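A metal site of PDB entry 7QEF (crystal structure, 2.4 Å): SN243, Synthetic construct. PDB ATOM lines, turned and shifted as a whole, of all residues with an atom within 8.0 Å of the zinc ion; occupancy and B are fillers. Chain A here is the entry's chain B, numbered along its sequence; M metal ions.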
ATOM      1  N   ILE A  22      12.262  -7.480 -11.931  1.00  0.00           N
ATOM      2  CA  ILE A  22      12.358  -7.985 -13.294  1.00  0.00           C
ATOM      3  C   ILE A  22      11.490  -7.093 -14.175  1.00  0.00           C
ATOM      4  O   ILE A  22      10.401  -6.680 -13.767  1.00  0.00           O
ATOM      5  CB  ILE A  22      11.964  -9.474 -13.430  1.00  0.00           C
ATOM      6  CG1 ILE A  22      10.475  -9.701 -13.184  1.00  0.00           C
ATOM      7  CG2 ILE A  22      12.826 -10.356 -12.531  1.00  0.00           C
ATOM      8  CD1 ILE A  22      10.114 -11.161 -13.236  1.00  0.00           C
ATOM      9  N   ARG A  30       8.269  -7.319  -8.832  1.00  0.00           N
ATOM     10  CA  ARG A  30       9.066  -8.023  -7.833  1.00  0.00           C
ATOM     11  C   ARG A  30       8.966  -9.514  -8.109  1.00  0.00           C
ATOM     12  O   ARG A  30       7.889 -10.094  -8.013  1.00  0.00           O
ATOM     13  CB  ARG A  30       8.592  -7.702  -6.403  1.00  0.00           C
ATOM     14  CG  ARG A  30       8.705  -6.235  -5.999  1.00  0.00           C
ATOM     15  CD  ARG A  30       8.892  -6.071  -4.490  1.00  0.00           C
ATOM     16  NE  ARG A  30       7.744  -6.544  -3.714  1.00  0.00           N
ATOM     17  CZ  ARG A  30       7.800  -6.980  -2.467  1.00  0.00           C
ATOM     18  NH1 ARG A  30       6.691  -7.380  -1.867  1.00  0.00           N
ATOM     19  NH2 ARG A  30       8.951  -7.022  -1.802  1.00  0.00           N
ATOM     20  N   ASP A  31      10.097 -10.140  -8.410  1.00  0.00           N
ATOM     21  CA  ASP A  31      10.078 -11.565  -8.702  1.00  0.00           C
ATOM     22  C   ASP A  31      10.223 -12.268  -7.357  1.00  0.00           C
ATOM     23  O   ASP A  31      11.329 -12.493  -6.875  1.00  0.00           O
ATOM     24  CB  ASP A  31      11.176 -11.968  -9.672  1.00  0.00           C
ATOM     25  CG  ASP A  31      11.088 -13.443 -10.101  1.00  0.00           C
ATOM     26  OD1 ASP A  31      10.181 -14.156  -9.631  1.00  0.00           O
ATOM     27  OD2 ASP A  31      11.932 -13.892 -10.893  1.00  0.00           O
ATOM     28  N   LEU A  32       9.083 -12.623  -6.769  1.00  0.00           N
ATOM     29  CA  LEU A  32       9.060 -13.085  -5.386  1.00  0.00           C
ATOM     30  C   LEU A  32       9.277 -14.574  -5.232  1.00  0.00           C
ATOM     31  O   LEU A  32       9.812 -14.985  -4.199  1.00  0.00           O
ATOM     32  CB  LEU A  32       7.747 -12.681  -4.720  1.00  0.00           C
ATOM     33  CG  LEU A  32       7.608 -11.164  -4.585  1.00  0.00           C
ATOM     34  CD1 LEU A  32       6.169 -10.738  -4.372  1.00  0.00           C
ATOM     35  CD2 LEU A  32       8.483 -10.599  -3.470  1.00  0.00           C
ATOM     36  N   ASN A  33       8.890 -15.422  -6.200  1.00  0.00           N
ATOM     37  CA  ASN A  33       9.277 -16.821  -6.075  1.00  0.00           C
ATOM     38  C   ASN A  33      10.715 -17.073  -6.515  1.00  0.00           C
ATOM     39  O   ASN A  33      11.214 -18.189  -6.318  1.00  0.00           O
ATOM     40  CB  ASN A  33       8.353 -17.795  -6.819  1.00  0.00           C
ATOM     41  CG  ASN A  33       7.812 -17.260  -8.116  1.00  0.00           C
ATOM     42  OD1 ASN A  33       8.503 -16.543  -8.829  1.00  0.00           O
ATOM     43  ND2 ASN A  33       6.592 -17.649  -8.453  1.00  0.00           N
ATOM     44  N   ASP A  34      11.368 -16.068  -7.127  1.00  0.00           N
ATOM     45  CA  ASP A  34      12.757 -16.166  -7.591  1.00  0.00           C
ATOM     46  C   ASP A  34      12.956 -17.323  -8.579  1.00  0.00           C
ATOM     47  O   ASP A  34      13.979 -18.002  -8.578  1.00  0.00           O
ATOM     48  CB  ASP A  34      13.714 -16.268  -6.400  1.00  0.00           C
ATOM     49  CG  ASP A  34      15.176 -16.128  -6.803  1.00  0.00           C
ATOM     50  OD1 ASP A  34      15.473 -15.286  -7.669  1.00  0.00           O
ATOM     51  OD2 ASP A  34      16.017 -16.879  -6.245  1.00  0.00           O
ATOM     52  N   ASN A  35      11.964 -17.533  -9.448  1.00  0.00           N
ATOM     53  CA  ASN A  35      12.135 -18.492 -10.536  1.00  0.00           C
ATOM     54  C   ASN A  35      12.666 -17.829 -11.802  1.00  0.00           C
ATOM     55  O   ASN A  35      13.128 -18.529 -12.703  1.00  0.00           O
ATOM     56  CB  ASN A  35      10.815 -19.221 -10.829  1.00  0.00           C
ATOM     57  CG  ASN A  35       9.706 -18.299 -11.326  1.00  0.00           C
ATOM     58  OD1 ASN A  35       9.932 -17.121 -11.580  1.00  0.00           O
ATOM     59  ND2 ASN A  35       8.500 -18.844 -11.452  1.00  0.00           N
ATOM     60  N   GLY A  36      12.592 -16.498 -11.873  1.00  0.00           N
ATOM     61  CA  GLY A  36      13.161 -15.720 -12.942  1.00  0.00           C
ATOM     62  C   GLY A  36      12.121 -15.150 -13.865  1.00  0.00           C
ATOM     63  O   GLY A  36      12.403 -14.204 -14.602  1.00  0.00           O
ATOM     64  N   GLU A  37      10.914 -15.704 -13.833  1.00  0.00           N
ATOM     65  CA  GLU A  37       9.828 -15.319 -14.711  1.00  0.00           C
ATOM     66  C   GLU A  37       8.769 -14.577 -13.908  1.00  0.00           C
ATOM     67  O   GLU A  37       8.665 -14.752 -12.690  1.00  0.00           O
ATOM     68  CB  GLU A  37       9.238 -16.551 -15.418  1.00  0.00           C
ATOM     69  CG  GLU A  37      10.280 -17.620 -15.817  1.00  0.00           C
ATOM     70  CD  GLU A  37      11.265 -17.161 -16.910  1.00  0.00           C
ATOM     71  OE1 GLU A  37      11.151 -16.029 -17.418  1.00  0.00           O
ATOM     72  OE2 GLU A  37      12.158 -17.972 -17.274  1.00  0.00           O
ATOM     73  N   LEU A  38       8.030 -13.714 -14.596  1.00  0.00           N
ATOM     74  CA  LEU A  38       6.878 -13.031 -14.006  1.00  0.00           C
ATOM     75  C   LEU A  38       5.714 -13.997 -13.848  1.00  0.00           C
ATOM     76  O   LEU A  38       5.066 -14.363 -14.832  1.00  0.00           O
ATOM     77  CB  LEU A  38       6.459 -11.861 -14.887  1.00  0.00           C
ATOM     78  CG  LEU A  38       5.389 -11.017 -14.207  1.00  0.00           C
ATOM     79  CD1 LEU A  38       6.049 -10.141 -13.169  1.00  0.00           C
ATOM     80  CD2 LEU A  38       4.615 -10.187 -15.214  1.00  0.00           C
ATOM     81  N   ASP A  39       5.366 -14.359 -12.578  1.00  0.00           N
ATOM     82  CA  ASP A  39       4.148 -15.115 -12.334  1.00  0.00           C
ATOM     83  C   ASP A  39       2.975 -14.157 -12.190  1.00  0.00           C
ATOM     84  O   ASP A  39       3.141 -13.005 -11.783  1.00  0.00           O
ATOM     85  CB  ASP A  39       4.277 -15.975 -11.072  1.00  0.00           C
ATOM     86  CG  ASP A  39       5.417 -16.979 -11.138  1.00  0.00           C
ATOM     87  OD1 ASP A  39       6.526 -16.603 -11.584  1.00  0.00           O
ATOM     88  OD2 ASP A  39       5.230 -18.157 -10.731  1.00  0.00           O
ATOM     89  N   PRO A  40       1.759 -14.616 -12.540  1.00  0.00           N
ATOM     90  CA  PRO A  40       0.576 -13.732 -12.427  1.00  0.00           C
ATOM     91  C   PRO A  40       0.398 -13.076 -11.056  1.00  0.00           C
ATOM     92  O   PRO A  40      -0.163 -11.973 -10.991  1.00  0.00           O
ATOM     93  CB  PRO A  40      -0.580 -14.680 -12.762  1.00  0.00           C
ATOM     94  CG  PRO A  40       0.026 -15.770 -13.575  1.00  0.00           C
ATOM     95  CD  PRO A  40       1.464 -15.893 -13.204  1.00  0.00           C
ATOM     96  N   TYR A  41       0.825 -13.722  -9.966  1.00  0.00           N
ATOM     97  CA  TYR A  41       0.604 -13.102  -8.646  1.00  0.00           C
ATOM     98  C   TYR A  41       1.572 -11.952  -8.379  1.00  0.00           C
ATOM     99  O   TYR A  41       1.267 -11.082  -7.548  1.00  0.00           O
ATOM    100  CB  TYR A  41       0.667 -14.161  -7.540  1.00  0.00           C
ATOM    101  CG  TYR A  41       2.019 -14.436  -6.939  1.00  0.00           C
ATOM    102  CD1 TYR A  41       2.549 -13.614  -5.934  1.00  0.00           C
ATOM    103  CD2 TYR A  41       2.745 -15.552  -7.320  1.00  0.00           C
ATOM    104  CE1 TYR A  41       3.779 -13.888  -5.381  1.00  0.00           C
ATOM    105  CE2 TYR A  41       3.972 -15.843  -6.755  1.00  0.00           C
ATOM    106  CZ  TYR A  41       4.480 -15.010  -5.778  1.00  0.00           C
ATOM    107  OH  TYR A  41       5.697 -15.289  -5.207  1.00  0.00           O
ATOM    108  N   GLU A  42       2.737 -11.942  -9.036  1.00  0.00           N
ATOM    109  CA  GLU A  42       3.626 -10.798  -8.986  1.00  0.00           C
ATOM    110  C   GLU A  42       3.207  -9.722  -9.974  1.00  0.00           C
ATOM    111  O   GLU A  42       3.611  -8.576  -9.817  1.00  0.00           O
ATOM    112  CB  GLU A  42       5.053 -11.265  -9.254  1.00  0.00           C
ATOM    113  CG  GLU A  42       5.200 -12.742  -8.855  1.00  0.00           C
ATOM    114  CD  GLU A  42       6.546 -13.342  -9.134  1.00  0.00           C
ATOM    115  OE1 GLU A  42       6.920 -13.437 -10.317  1.00  0.00           O
ATOM    116  OE2 GLU A  42       7.222 -13.754  -8.157  1.00  0.00           O
ATOM    117  N   ASP A  43       2.327 -10.063 -10.912  1.00  0.00           N
ATOM    118  CA  ASP A  43       1.877  -9.151 -11.964  1.00  0.00           C
ATOM    119  C   ASP A  43       0.809  -8.230 -11.377  1.00  0.00           C
ATOM    120  O   ASP A  43      -0.350  -8.630 -11.229  1.00  0.00           O
ATOM    121  CB  ASP A  43       1.358  -9.956 -13.159  1.00  0.00           C
ATOM    122  CG  ASP A  43       0.982  -9.095 -14.366  1.00  0.00           C
ATOM    123  OD1 ASP A  43       0.935  -7.849 -14.256  1.00  0.00           O
ATOM    124  OD2 ASP A  43       0.728  -9.696 -15.443  1.00  0.00           O
ATOM    125  N   ASP A  54      -3.278 -17.480  -8.618  1.00  0.00           N
ATOM    126  CA  ASP A  54      -1.969 -17.976  -9.003  1.00  0.00           C
ATOM    127  C   ASP A  54      -1.101 -18.285  -7.779  1.00  0.00           C
ATOM    128  O   ASP A  54      -0.397 -19.294  -7.756  1.00  0.00           O
ATOM    129  CB  ASP A  54      -1.290 -16.965  -9.926  1.00  0.00           C
ATOM    130  CG  ASP A  54       0.063 -17.435 -10.427  1.00  0.00           C
ATOM    131  OD1 ASP A  54       0.121 -18.326 -11.313  1.00  0.00           O
ATOM    132  OD2 ASP A  54       1.079 -16.895  -9.941  1.00  0.00           O
ATOM    133  N   GLN A  58       0.368 -22.036  -6.325  1.00  0.00           N
ATOM    134  CA  GLN A  58       1.773 -22.355  -6.106  1.00  0.00           C
ATOM    135  C   GLN A  58       2.097 -22.712  -4.650  1.00  0.00           C
ATOM    136  O   GLN A  58       3.262 -23.008  -4.344  1.00  0.00           O
ATOM    137  CB  GLN A  58       2.655 -21.156  -6.483  1.00  0.00           C
ATOM    138  CG  GLN A  58       2.515 -20.682  -7.876  1.00  0.00           C
ATOM    139  CD  GLN A  58       3.474 -19.557  -8.179  1.00  0.00           C
ATOM    140  OE1 GLN A  58       4.676 -19.635  -7.863  1.00  0.00           O
ATOM    141  NE2 GLN A  58       2.963 -18.510  -8.837  1.00  0.00           N
HETATM  142 ZN    ZN M   1       8.255 -15.244 -10.709  1.00  0.00          ZN
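OD1 of Asn 35 is in hydrogen-bond range of N of Glu 37, 2.8 Å away.
The backbone NH (N) of Leu 32 sits at hydrogen-bond distance from the side-chain carboxylate (OE2) of Glu 42 (2.6 Å).
OD1 of Asn 33 sits close to OD1 of Asn 35 (3.2 Å).
The backbone NH (N) of Asn 33 is in hydrogen-bond range of the side-chain hydroxyl (OH) of Tyr 41.
The side-chain carboxylate (OD2) of Asp 39 sits at hydrogen-bond distance from the side-chain amide nitrogen (ND2) of Asn 35 (3.4 Å).
The side-chain carboxylate (OD2) of Asp 39 is in hydrogen-bond range of the side-chain amide nitrogen (NE2) of Gln 58, 3.0 Å away.
The side-chain carboxylate of Asp 31 is in hydrogen-bond range of the backbone NH of Gly 36 (2.9 Å).
The side-chain carboxylate (OD1) of Asp 31 lies close to the backbone NH (N) of Asp 34, at 3.4 Å.
Of the 17 residues printed, 6 come within 4 Å of the zinc ion.
Along chain A the residues within 4 Å of the zinc ion span positions 31 to 42.
The nearest printed residue that does not touch the zinc ion is Leu 38 (4.2 Å).
The zinc ion is bound by the backbone carbonyl oxygen (O) of Glu 37 (2.1 Å), the side-chain carboxylate (OE1) of Glu 42 (2.3 Å), the side-chain amide oxygen (OD1) of Asn 33 (2.3 Å), the side-chain carboxylate (OD1) of Asp 39 (2.4 Å) and the side-chain carboxylate (OD1) of Asp 31 (2.5 Å).
The zinc ion has five donor atoms within binding distance.
Slightly farther from the zinc ion lies OD1 of Asn 35 (2.7 Å).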
